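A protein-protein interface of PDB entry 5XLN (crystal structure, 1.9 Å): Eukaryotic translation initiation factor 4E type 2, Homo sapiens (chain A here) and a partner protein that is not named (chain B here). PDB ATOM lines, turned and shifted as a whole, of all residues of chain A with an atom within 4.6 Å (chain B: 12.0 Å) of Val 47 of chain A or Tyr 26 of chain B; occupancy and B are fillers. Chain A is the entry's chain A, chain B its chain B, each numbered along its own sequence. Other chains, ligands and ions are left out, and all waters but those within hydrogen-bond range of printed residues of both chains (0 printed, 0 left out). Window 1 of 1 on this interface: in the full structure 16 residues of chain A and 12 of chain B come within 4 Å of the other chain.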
ATOM      1  N   HIS A  10      26.600  19.179 -16.110  1.00  0.00           N
ATOM      2  CA  HIS A  10      26.245  18.295 -17.217  1.00  0.00           C
ATOM      3  C   HIS A  10      24.727  18.238 -17.345  1.00  0.00           C
ATOM      4  O   HIS A  10      24.074  17.592 -16.542  1.00  0.00           O
ATOM      5  CB  HIS A  10      26.826  16.874 -16.998  1.00  0.00           C
ATOM      6  CG  HIS A  10      28.322  16.818 -17.077  1.00  0.00           C
ATOM      7  ND1 HIS A  10      29.135  17.266 -16.061  1.00  0.00           N
ATOM      8  CD2 HIS A  10      29.150  16.402 -18.068  1.00  0.00           C
ATOM      9  CE1 HIS A  10      30.403  17.114 -16.413  1.00  0.00           C
ATOM     10  NE2 HIS A  10      30.438  16.597 -17.627  1.00  0.00           N
ATOM     11  N   PRO A  11      24.162  18.922 -18.351  1.00  0.00           N
ATOM     12  CA  PRO A  11      22.701  19.011 -18.457  1.00  0.00           C
ATOM     13  C   PRO A  11      22.030  17.669 -18.710  1.00  0.00           C
ATOM     14  O   PRO A  11      22.627  16.779 -19.310  1.00  0.00           O
ATOM     15  CB  PRO A  11      22.478  19.932 -19.674  1.00  0.00           C
ATOM     16  CG  PRO A  11      23.804  20.598 -19.927  1.00  0.00           C
ATOM     17  CD  PRO A  11      24.839  19.611 -19.467  1.00  0.00           C
ATOM     18  N   LEU A  12      20.784  17.552 -18.271  1.00  0.00           N
ATOM     19  CA  LEU A  12      19.961  16.395 -18.585  1.00  0.00           C
ATOM     20  C   LEU A  12      19.063  16.736 -19.771  1.00  0.00           C
ATOM     21  O   LEU A  12      18.825  17.909 -20.062  1.00  0.00           O
ATOM     22  CB  LEU A  12      19.109  15.974 -17.379  1.00  0.00           C
ATOM     23  CG  LEU A  12      19.862  15.518 -16.115  1.00  0.00           C
ATOM     24  CD1 LEU A  12      18.877  15.333 -14.965  1.00  0.00           C
ATOM     25  CD2 LEU A  12      20.596  14.225 -16.379  1.00  0.00           C
ATOM     26  N   SER A  46      20.380  18.675 -14.034  1.00  0.00           N
ATOM     27  CA  SER A  46      21.718  18.259 -14.421  1.00  0.00           C
ATOM     28  C   SER A  46      22.126  17.022 -13.624  1.00  0.00           C
ATOM     29  O   SER A  46      21.515  16.704 -12.596  1.00  0.00           O
ATOM     30  CB  SER A  46      22.728  19.387 -14.195  1.00  0.00           C
ATOM     31  OG  SER A  46      22.889  19.648 -12.807  1.00  0.00           O
ATOM     32  N   VAL A  47      23.163  16.340 -14.100  1.00  0.00           N
ATOM     33  CA  VAL A  47      23.682  15.179 -13.378  1.00  0.00           C
ATOM     34  C   VAL A  47      24.158  15.576 -11.977  1.00  0.00           C
ATOM     35  O   VAL A  47      23.916  14.851 -11.007  1.00  0.00           O
ATOM     36  CB  VAL A  47      24.834  14.523 -14.130  1.00  0.00           C
ATOM     37  CG1 VAL A  47      25.300  13.275 -13.380  1.00  0.00           C
ATOM     38  CG2 VAL A  47      24.397  14.159 -15.561  1.00  0.00           C
ATOM     39  N   GLU A  48      24.811  16.733 -11.865  1.00  0.00           N
ATOM     40  CA  GLU A  48      25.327  17.176 -10.564  1.00  0.00           C
ATOM     41  C   GLU A  48      24.180  17.451  -9.591  1.00  0.00           C
ATOM     42  O   GLU A  48      24.232  17.032  -8.428  1.00  0.00           O
ATOM     43  CB  GLU A  48      26.218  18.422 -10.720  1.00  0.00           C
ATOM     44  CG  GLU A  48      27.585  18.144 -11.375  1.00  0.00           C
ATOM     45  CD  GLU A  48      27.562  18.162 -12.907  1.00  0.00           C
ATOM     46  OE1 GLU A  48      26.465  18.134 -13.519  1.00  0.00           O
ATOM     47  OE2 GLU A  48      28.658  18.206 -13.508  1.00  0.00           O
ATOM     48  N   GLN A  49      23.138  18.138 -10.061  1.00  0.00           N
ATOM     49  CA  GLN A  49      21.976  18.405  -9.208  1.00  0.00           C
ATOM     50  C   GLN A  49      21.302  17.109  -8.782  1.00  0.00           C
ATOM     51  O   GLN A  49      20.800  16.997  -7.656  1.00  0.00           O
ATOM     52  CB  GLN A  49      20.954  19.307  -9.925  1.00  0.00           C
ATOM     53  CG  GLN A  49      21.422  20.749 -10.064  1.00  0.00           C
ATOM     54  CD  GLN A  49      20.536  21.550 -10.996  1.00  0.00           C
ATOM     55  OE1 GLN A  49      19.374  21.208 -11.218  1.00  0.00           O
ATOM     56  NE2 GLN A  49      21.084  22.622 -11.550  1.00  0.00           N
ATOM     57  N   PHE A  50      21.270  16.134  -9.688  1.00  0.00           N
ATOM     58  CA  PHE A  50      20.701  14.832  -9.352  1.00  0.00           C
ATOM     59  C   PHE A  50      21.436  14.197  -8.172  1.00  0.00           C
ATOM     60  O   PHE A  50      20.819  13.756  -7.199  1.00  0.00           O
ATOM     61  CB  PHE A  50      20.751  13.857 -10.542  1.00  0.00           C
ATOM     62  CG  PHE A  50      20.690  12.407 -10.114  1.00  0.00           C
ATOM     63  CD1 PHE A  50      19.515  11.873  -9.598  1.00  0.00           C
ATOM     64  CD2 PHE A  50      21.814  11.598 -10.184  1.00  0.00           C
ATOM     65  CE1 PHE A  50      19.455  10.542  -9.182  1.00  0.00           C
ATOM     66  CE2 PHE A  50      21.766  10.261  -9.764  1.00  0.00           C
ATOM     67  CZ  PHE A  50      20.587   9.737  -9.265  1.00  0.00           C
ATOM     68  N   TRP A  51      22.753  14.116  -8.279  1.00  0.00           N
ATOM     69  CA  TRP A  51      23.536  13.490  -7.217  1.00  0.00           C
ATOM     70  C   TRP A  51      23.388  14.252  -5.895  1.00  0.00           C
ATOM     71  O   TRP A  51      23.377  13.656  -4.819  1.00  0.00           O
ATOM     72  CB  TRP A  51      25.009  13.409  -7.600  1.00  0.00           C
ATOM     73  CG  TRP A  51      25.342  12.347  -8.616  1.00  0.00           C
ATOM     74  CD1 TRP A  51      25.911  12.546  -9.844  1.00  0.00           C
ATOM     75  CD2 TRP A  51      25.147  10.925  -8.490  1.00  0.00           C
ATOM     76  NE1 TRP A  51      26.087  11.337 -10.487  1.00  0.00           N
ATOM     77  CE2 TRP A  51      25.624  10.328  -9.680  1.00  0.00           C
ATOM     78  CE3 TRP A  51      24.628  10.099  -7.484  1.00  0.00           C
ATOM     79  CZ2 TRP A  51      25.589   8.946  -9.897  1.00  0.00           C
ATOM     80  CZ3 TRP A  51      24.591   8.721  -7.700  1.00  0.00           C
ATOM     81  CH2 TRP A  51      25.073   8.159  -8.901  1.00  0.00           C
ATOM     82  N   GLY A 113      20.142   9.036 -17.986  1.00  0.00           N
ATOM     83  CA  GLY A 113      21.173   9.079 -19.016  1.00  0.00           C
ATOM     84  C   GLY A 113      20.664   8.742 -20.409  1.00  0.00           C
ATOM     85  O   GLY A 113      21.463   8.549 -21.331  1.00  0.00           O
ATOM     86  N   GLN A 115      19.283   6.082 -21.657  1.00  0.00           N
ATOM     87  CA  GLN A 115      19.726   4.787 -22.148  1.00  0.00           C
ATOM     88  C   GLN A 115      18.612   3.967 -22.814  1.00  0.00           C
ATOM     89  O   GLN A 115      18.901   3.001 -23.526  1.00  0.00           O
ATOM     90  CB  GLN A 115      20.352   3.993 -20.994  1.00  0.00           C
ATOM     91  CG  GLN A 115      21.689   4.579 -20.529  1.00  0.00           C
ATOM     92  CD  GLN A 115      22.746   4.485 -21.613  1.00  0.00           C
ATOM     93  OE1 GLN A 115      22.934   3.427 -22.204  1.00  0.00           O
ATOM     94  NE2 GLN A 115      23.410   5.594 -21.904  1.00  0.00           N
ATOM     95  N   TRP B  21      19.166  11.489 -32.308  1.00  0.00           N
ATOM     96  CA  TRP B  21      19.447  11.137 -30.922  1.00  0.00           C
ATOM     97  C   TRP B  21      19.201  12.325 -29.995  1.00  0.00           C
ATOM     98  O   TRP B  21      19.145  13.471 -30.450  1.00  0.00           O
ATOM     99  CB  TRP B  21      20.894  10.649 -30.777  1.00  0.00           C
ATOM    100  CG  TRP B  21      21.108   9.216 -31.175  1.00  0.00           C
ATOM    101  CD1 TRP B  21      20.186   8.363 -31.708  1.00  0.00           C
ATOM    102  CD2 TRP B  21      22.328   8.469 -31.060  1.00  0.00           C
ATOM    103  NE1 TRP B  21      20.755   7.132 -31.937  1.00  0.00           N
ATOM    104  CE2 TRP B  21      22.067   7.171 -31.548  1.00  0.00           C
ATOM    105  CE3 TRP B  21      23.612   8.772 -30.596  1.00  0.00           C
ATOM    106  CZ2 TRP B  21      23.049   6.176 -31.583  1.00  0.00           C
ATOM    107  CZ3 TRP B  21      24.584   7.782 -30.632  1.00  0.00           C
ATOM    108  CH2 TRP B  21      24.296   6.502 -31.123  1.00  0.00           C
ATOM    109  N   PRO B  22      19.039  12.057 -28.690  1.00  0.00           N
ATOM    110  CA  PRO B  22      19.024  13.177 -27.745  1.00  0.00           C
ATOM    111  C   PRO B  22      20.408  13.798 -27.619  1.00  0.00           C
ATOM    112  O   PRO B  22      21.401  13.129 -27.888  1.00  0.00           O
ATOM    113  CB  PRO B  22      18.591  12.526 -26.426  1.00  0.00           C
ATOM    114  CG  PRO B  22      18.946  11.097 -26.580  1.00  0.00           C
ATOM    115  CD  PRO B  22      18.741  10.774 -28.028  1.00  0.00           C
ATOM    116  N   GLU B  23      20.471  15.058 -27.208  1.00  0.00           N
ATOM    117  CA  GLU B  23      21.752  15.724 -27.028  1.00  0.00           C
ATOM    118  C   GLU B  23      22.504  15.151 -25.834  1.00  0.00           C
ATOM    119  O   GLU B  23      23.727  15.021 -25.860  1.00  0.00           O
ATOM    120  CB  GLU B  23      21.555  17.226 -26.824  1.00  0.00           C
ATOM    121  CG  GLU B  23      20.488  17.860 -27.692  1.00  0.00           C
ATOM    122  CD  GLU B  23      21.012  19.063 -28.453  1.00  0.00           C
ATOM    123  OE1 GLU B  23      22.039  19.638 -28.023  1.00  0.00           O
ATOM    124  OE2 GLU B  23      20.394  19.440 -29.473  1.00  0.00           O
ATOM    125  N   TYR B  24      21.758  14.805 -24.787  1.00  0.00           N
ATOM    126  CA  TYR B  24      22.363  14.511 -23.486  1.00  0.00           C
ATOM    127  C   TYR B  24      22.198  13.061 -23.084  1.00  0.00           C
ATOM    128  O   TYR B  24      21.231  12.680 -22.436  1.00  0.00           O
ATOM    129  CB  TYR B  24      21.781  15.464 -22.425  1.00  0.00           C
ATOM    130  CG  TYR B  24      22.081  16.901 -22.780  1.00  0.00           C
ATOM    131  CD1 TYR B  24      23.389  17.379 -22.753  1.00  0.00           C
ATOM    132  CD2 TYR B  24      21.072  17.772 -23.180  1.00  0.00           C
ATOM    133  CE1 TYR B  24      23.683  18.690 -23.102  1.00  0.00           C
ATOM    134  CE2 TYR B  24      21.357  19.097 -23.531  1.00  0.00           C
ATOM    135  CZ  TYR B  24      22.668  19.543 -23.488  1.00  0.00           C
ATOM    136  OH  TYR B  24      22.981  20.842 -23.828  1.00  0.00           O
ATOM    137  N   ILE B  25      23.174  12.258 -23.497  1.00  0.00           N
ATOM    138  CA  ILE B  25      23.225  10.829 -23.212  1.00  0.00           C
ATOM    139  C   ILE B  25      24.395  10.548 -22.278  1.00  0.00           C
ATOM    140  O   ILE B  25      25.507  11.023 -22.512  1.00  0.00           O
ATOM    141  CB  ILE B  25      23.391  10.002 -24.517  1.00  0.00           C
ATOM    142  CG1 ILE B  25      22.208  10.237 -25.451  1.00  0.00           C
ATOM    143  CG2 ILE B  25      23.511   8.523 -24.222  1.00  0.00           C
ATOM    144  CD1 ILE B  25      22.380   9.604 -26.823  1.00  0.00           C
ATOM    145  N   TYR B  26      24.149   9.797 -21.213  1.00  0.00           N
ATOM    146  CA  TYR B  26      25.215   9.472 -20.268  1.00  0.00           C
ATOM    147  C   TYR B  26      25.217   7.988 -19.974  1.00  0.00           C
ATOM    148  O   TYR B  26      24.178   7.416 -19.644  1.00  0.00           O
ATOM    149  CB  TYR B  26      25.057  10.251 -18.955  1.00  0.00           C
ATOM    150  CG  TYR B  26      25.051  11.746 -19.149  1.00  0.00           C
ATOM    151  CD1 TYR B  26      26.237  12.446 -19.325  1.00  0.00           C
ATOM    152  CD2 TYR B  26      23.849  12.457 -19.192  1.00  0.00           C
ATOM    153  CE1 TYR B  26      26.233  13.816 -19.517  1.00  0.00           C
ATOM    154  CE2 TYR B  26      23.834  13.819 -19.384  1.00  0.00           C
ATOM    155  CZ  TYR B  26      25.028  14.496 -19.545  1.00  0.00           C
ATOM    156  OH  TYR B  26      25.012  15.855 -19.748  1.00  0.00           O
ATOM    157  N   THR B  27      26.380   7.366 -20.100  1.00  0.00           N
ATOM    158  CA  THR B  27      26.518   5.976 -19.692  1.00  0.00           C
ATOM    159  C   THR B  27      26.538   5.910 -18.174  1.00  0.00           C
ATOM    160  O   THR B  27      26.747   6.926 -17.500  1.00  0.00           O
ATOM    161  CB  THR B  27      27.806   5.327 -20.238  1.00  0.00           C
ATOM    162  OG1 THR B  27      28.943   5.986 -19.658  1.00  0.00           O
ATOM    163  CG2 THR B  27      27.854   5.431 -21.756  1.00  0.00           C
ATOM    164  N   ARG B  28      26.338   4.718 -17.629  1.00  0.00           N
ATOM    165  CA  ARG B  28      26.393   4.561 -16.182  1.00  0.00           C
ATOM    166  C   ARG B  28      27.748   5.012 -15.631  1.00  0.00           C
ATOM    167  O   ARG B  28      27.819   5.682 -14.600  1.00  0.00           O
ATOM    168  CB  ARG B  28      26.105   3.107 -15.791  1.00  0.00           C
ATOM    169  CG  ARG B  28      26.306   2.830 -14.318  1.00  0.00           C
ATOM    170  CD  ARG B  28      25.265   1.853 -13.762  1.00  0.00           C
ATOM    171  NE  ARG B  28      25.704   0.463 -13.808  1.00  0.00           N
ATOM    172  CZ  ARG B  28      24.975  -0.564 -14.261  1.00  0.00           C
ATOM    173  NH1 ARG B  28      23.728  -0.396 -14.721  1.00  0.00           N
ATOM    174  NH2 ARG B  28      25.500  -1.781 -14.245  1.00  0.00           N
ATOM    175  N   LEU B  29      28.823   4.667 -16.333  1.00  0.00           N
ATOM    176  CA  LEU B  29      30.162   5.068 -15.899  1.00  0.00           C
ATOM    177  C   LEU B  29      30.331   6.591 -15.933  1.00  0.00           C
ATOM    178  O   LEU B  29      30.938   7.177 -15.037  1.00  0.00           O
ATOM    179  CB  LEU B  29      31.234   4.405 -16.768  1.00  0.00           C
ATOM    180  CG  LEU B  29      32.679   4.779 -16.425  1.00  0.00           C
ATOM    181  CD1 LEU B  29      33.010   4.456 -14.965  1.00  0.00           C
ATOM    182  CD2 LEU B  29      33.653   4.082 -17.369  1.00  0.00           C
ATOM    183  N   GLU B  30      29.797   7.224 -16.967  1.00  0.00           N
ATOM    184  CA  GLU B  30      29.836   8.684 -17.045  1.00  0.00           C
ATOM    185  C   GLU B  30      29.071   9.329 -15.875  1.00  0.00           C
ATOM    186  O   GLU B  30      29.535  10.314 -15.307  1.00  0.00           O
ATOM    187  CB  GLU B  30      29.289   9.154 -18.395  1.00  0.00           C
ATOM    188  CG  GLU B  30      30.277   8.890 -19.511  1.00  0.00           C
ATOM    189  CD  GLU B  30      29.735   9.182 -20.893  1.00  0.00           C
ATOM    190  OE1 GLU B  30      28.513   9.049 -21.124  1.00  0.00           O
ATOM    191  OE2 GLU B  30      30.552   9.543 -21.756  1.00  0.00           O
ATOM    192  N   MET B  31      27.928   8.763 -15.497  1.00  0.00           N
ATOM    193  CA  MET B  31      27.184   9.269 -14.338  1.00  0.00           C
ATOM    194  C   MET B  31      28.056   9.203 -13.078  1.00  0.00           C
ATOM    195  O   MET B  31      28.115  10.157 -12.305  1.00  0.00           O
ATOM    196  CB  MET B  31      25.886   8.481 -14.115  1.00  0.00           C
ATOM    197  CG  MET B  31      24.884   8.566 -15.273  1.00  0.00           C
ATOM    198  SD  MET B  31      24.191  10.210 -15.472  1.00  0.00           S
ATOM    199  CE  MET B  31      22.967  10.251 -14.145  1.00  0.00           C
ATOM    200  N   TYR B  32      28.755   8.088 -12.884  1.00  0.00           N
ATOM    201  CA  TYR B  32      29.583   7.948 -11.689  1.00  0.00           C
ATOM    202  C   TYR B  32      30.858   8.800 -11.754  1.00  0.00           C
ATOM    203  O   TYR B  32      31.353   9.237 -10.717  1.00  0.00           O
ATOM    204  CB  TYR B  32      29.945   6.477 -11.440  1.00  0.00           C
ATOM    205  CG  TYR B  32      28.795   5.642 -10.889  1.00  0.00           C
ATOM    206  CD1 TYR B  32      28.255   5.901  -9.634  1.00  0.00           C
ATOM    207  CD2 TYR B  32      28.274   4.587 -11.614  1.00  0.00           C
ATOM    208  CE1 TYR B  32      27.207   5.126  -9.122  1.00  0.00           C
ATOM    209  CE2 TYR B  32      27.236   3.806 -11.113  1.00  0.00           C
ATOM    210  CZ  TYR B  32      26.707   4.080  -9.871  1.00  0.00           C
ATOM    211  OH  TYR B  32      25.674   3.298  -9.390  1.00  0.00           O
ATOM    212  N   ASN B  33      31.386   9.036 -12.957  1.00  0.00           N
ATOM    213  CA  ASN B  33      32.546   9.926 -13.103  1.00  0.00           C
ATOM    214  C   ASN B  33      32.192  11.338 -12.626  1.00  0.00           C
ATOM    215  O   ASN B  33      32.989  12.020 -11.987  1.00  0.00           O
ATOM    216  CB  ASN B  33      33.038   9.982 -14.554  1.00  0.00           C
ATOM    217  CG  ASN B  33      33.768   8.722 -14.984  1.00  0.00           C
ATOM    218  OD1 ASN B  33      34.161   7.904 -14.155  1.00  0.00           O
ATOM    219  ND2 ASN B  33      33.961   8.570 -16.294  1.00  0.00           N
ATOM    220  N   ILE B  34      30.976  11.761 -12.943  1.00  0.00           N
ATOM    221  CA  ILE B  34      30.473  13.060 -12.518  1.00  0.00           C
ATOM    222  C   ILE B  34      30.272  13.088 -10.996  1.00  0.00           C
ATOM    223  O   ILE B  34      30.560  14.098 -10.348  1.00  0.00           O
ATOM    224  CB  ILE B  34      29.162  13.400 -13.286  1.00  0.00           C
ATOM    225  CG1 ILE B  34      29.472  13.478 -14.787  1.00  0.00           C
ATOM    226  CG2 ILE B  34      28.523  14.702 -12.762  1.00  0.00           C
ATOM    227  CD1 ILE B  34      28.251  13.564 -15.708  1.00  0.00           C
ATOM    228  N   LEU B  35      29.804  11.980 -10.420  1.00  0.00           N
ATOM    229  CA  LEU B  35      29.662  11.888  -8.969  1.00  0.00           C
ATOM    230  C   LEU B  35      31.023  12.057  -8.277  1.00  0.00           C
ATOM    231  O   LEU B  35      31.151  12.771  -7.273  1.00  0.00           O
ATOM    232  CB  LEU B  35      29.031  10.554  -8.574  1.00  0.00           C
ATOM    233  CG  LEU B  35      28.998  10.271  -7.069  1.00  0.00           C
ATOM    234  CD1 LEU B  35      28.085  11.287  -6.348  1.00  0.00           C
ATOM    235  CD2 LEU B  35      28.562   8.833  -6.805  1.00  0.00           C
ATOM    236  N   LYS B  36      32.042  11.415  -8.835  1.00  0.00           N
ATOM    237  CA  LYS B  36      33.391  11.516  -8.273  1.00  0.00           C
ATOM    238  C   LYS B  36      33.859  12.971  -8.255  1.00  0.00           C
ATOM    239  O   LYS B  36      34.403  13.448  -7.255  1.00  0.00           O
ATOM    240  CB  LYS B  36      34.375  10.657  -9.069  1.00  0.00           C
ATOM    241  CG  LYS B  36      35.837  10.981  -8.772  1.00  0.00           C
ATOM    242  CD  LYS B  36      36.792  10.179  -9.642  1.00  0.00           C
ATOM    243  CE  LYS B  36      38.244  10.474  -9.281  1.00  0.00           C
ATOM    244  NZ  LYS B  36      39.184   9.890 -10.278  1.00  0.00           N
ATOM    245  N   ALA B  37      33.624  13.680  -9.359  1.00  0.00           N
ATOM    246  CA  ALA B  37      34.015  15.082  -9.465  1.00  0.00           C
ATOM    247  C   ALA B  37      33.292  15.914  -8.413  1.00  0.00           C
ATOM    248  O   ALA B  37      33.893  16.754  -7.743  1.00  0.00           O
ATOM    249  CB  ALA B  37      33.721  15.613 -10.848  1.00  0.00           C
ATOM    250  N   GLU B  38      31.996  15.661  -8.271  1.00  0.00           N
ATOM    251  CA  GLU B  38      31.173  16.364  -7.299  1.00  0.00           C
ATOM    252  C   GLU B  38      31.654  16.106  -5.866  1.00  0.00           C
ATOM    253  O   GLU B  38      31.710  17.019  -5.043  1.00  0.00           O
ATOM    254  CB  GLU B  38      29.707  15.943  -7.460  1.00  0.00           C
ATOM    255  CG  GLU B  38      28.765  16.570  -6.458  1.00  0.00           C
ATOM    256  CD  GLU B  38      28.429  18.011  -6.791  1.00  0.00           C
ATOM    257  OE1 GLU B  38      28.885  18.512  -7.842  1.00  0.00           O
ATOM    258  OE2 GLU B  38      27.707  18.640  -5.994  1.00  0.00           O
ATOM    259  N   HIS B  39      32.014  14.859  -5.582  1.00  0.00           N
ATOM    260  CA  HIS B  39      32.469  14.472  -4.253  1.00  0.00           C
ATOM    261  C   HIS B  39      33.738  15.229  -3.849  1.00  0.00           C
ATOM    262  O   HIS B  39      33.892  15.624  -2.696  1.00  0.00           O
ATOM    263  CB  HIS B  39      32.707  12.958  -4.198  1.00  0.00           C
ATOM    264  CG  HIS B  39      33.252  12.472  -2.892  1.00  0.00           C
ATOM    265  ND1 HIS B  39      34.553  12.692  -2.494  1.00  0.00           N
ATOM    266  CD2 HIS B  39      32.672  11.763  -1.892  1.00  0.00           C
ATOM    267  CE1 HIS B  39      34.751  12.150  -1.307  1.00  0.00           C
ATOM    268  NE2 HIS B  39      33.623  11.579  -0.920  1.00  0.00           N
ATOM    269  N   SER B  41      34.798  18.181  -4.752  1.00  0.00           N
ATOM    270  CA  SER B  41      34.745  19.639  -4.797  1.00  0.00           C
ATOM    271  C   SER B  41      34.571  20.289  -3.417  1.00  0.00           C
ATOM    272  O   SER B  41      34.029  21.389  -3.312  1.00  0.00           O
ATOM    273  CB  SER B  41      33.628  20.098  -5.742  1.00  0.00           C
ATOM    274  OG  SER B  41      32.365  19.622  -5.314  1.00  0.00           O
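Val 47 of chain A touches just these residues of chain B: Tyr 26 (3.9 Å), Met 31 (3.9 Å) and Ile 34 (3.6 Å).
Tyr 26 of chain B touches five residues of chain A.
Of chain B, only Tyr 26 and Ile 34 come within 4 Å of His 10 of chain A.
Printed residues of chain B within 4 Å of Pro 11 of chain A: Tyr 24 (3.5 Å) and Tyr 26 (2.6 Å).
Of chain B, only Tyr 24 (3.8 Å) comes within 4 Å of Leu 12 of chain A.
Ser 46 of chain A touches none of the printed residues of chain B.
Of chain B, only Ile 34 (3.6 Å) and Glu 38 (3.8 Å) come within 4 Å of Glu 48 of chain A.
No residue of chain B comes within 4 Å of Gln 49 of chain A.
No residue of chain B comes within 4 Å of Phe 50 of chain A.
Trp 51 of chain A touches just these residues of chain B: Met 31, Tyr 32 and Leu 35.
Gln 115 of chain A touches just these residues of chain B: Ile 25, Tyr 26 and Thr 27.
Of the printed residues of chain A, Ile 34 of chain B touches His 10 (3.5 Å), Val 47 (3.6 Å) and Glu 48 (3.6 Å).
Of the printed residues of chain A, Tyr 24 of chain B touches Pro 11 (3.5 Å) and Leu 12 (3.8 Å).
Glu 30 of chain B touches none of the printed residues of chain A.
The nearest residue of chain A that does not touch Tyr 26 of chain B is Leu 12 of chain A (4.4 Å).
The nearest printed residue of chain A that does not touch Ile 25 of chain B is Pro 11 of chain A (6.2 Å).
Among the printed residues, pairs that only touch across the chains: His 10 of chain A with Tyr 26 of chain B (3.4 Å), Gly 113 of chain A with Ile 25 of chain B (3.4 Å), Pro 11 of chain A with Tyr 24 of chain B (3.5 Å), His 10 of chain A with Ile 34 of chain B (3.5 Å), Val 47 of chain A with Ile 34 of chain B (3.6 Å), Glu 48 of chain A with Ile 34 of chain B (3.6 Å), Trp 51 of chain A with Leu 35 of chain B (3.6 Å), Trp 51 of chain A with Tyr 32 of chain B (3.7 Å), Gln 115 of chain A with Ile 25 of chain B (3.7 Å), Glu 48 of chain A with Glu 38 of chain B (3.8 Å), Gln 115 of chain A with Thr 27 of chain B (3.8 Å), Leu 12 of chain A with Tyr 24 of chain B (3.8 Å), Val 47 of chain A with Met 31 of chain B (3.9 Å) and Val 47 of chain A with Tyr 26 of chain B (3.9 Å).
Of the 11 printed residues of chain A, 8 touch a printed residue of chain B.
Of the 20 printed residues of chain B, 9 touch a printed residue of chain A.
Among the printed residues, no Asp or Glu carboxylate lies within 4 Å of a Lys or Arg side-chain nitrogen of the other chain.
The backbone carbonyl oxygen of Pro 11 of chain A sits at hydrogen-bond distance from the side-chain hydroxyl of Tyr 26 of chain B, at 2.6 Å.
The indole nitrogen (NE1) of Trp 51 of chain A is in hydrogen-bond range of the backbone carbonyl oxygen (O) of Met 31 of chain B (3.0 Å).
The backbone NH of Tyr 26 of chain B sits at hydrogen-bond distance from the backbone carbonyl oxygen of Gly 113 of chain A.
The side-chain amide nitrogen (NE2) of Gln 115 of chain A sits at hydrogen-bond distance from the backbone carbonyl oxygen (O) of Tyr 26 of chain B, at 3.0 Å.
O of His 10 of chain A lies within hydrogen-bond range of N of Val 47 of chain A, 2.9 Å away.
A ring nitrogen (ND1) of His 10 of chain A is in hydrogen-bond range of the side-chain carboxylate (OE2) of Glu 48 of chain A.
The backbone NH of Thr 27 of chain B sits at hydrogen-bond distance from the side-chain carboxylate of Glu 30 of chain B.
The side-chain hydroxyl (OG) of Ser 41 of chain B is in hydrogen-bond range of the backbone carbonyl oxygen (O) of Glu 38 of chain B (2.7 Å).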
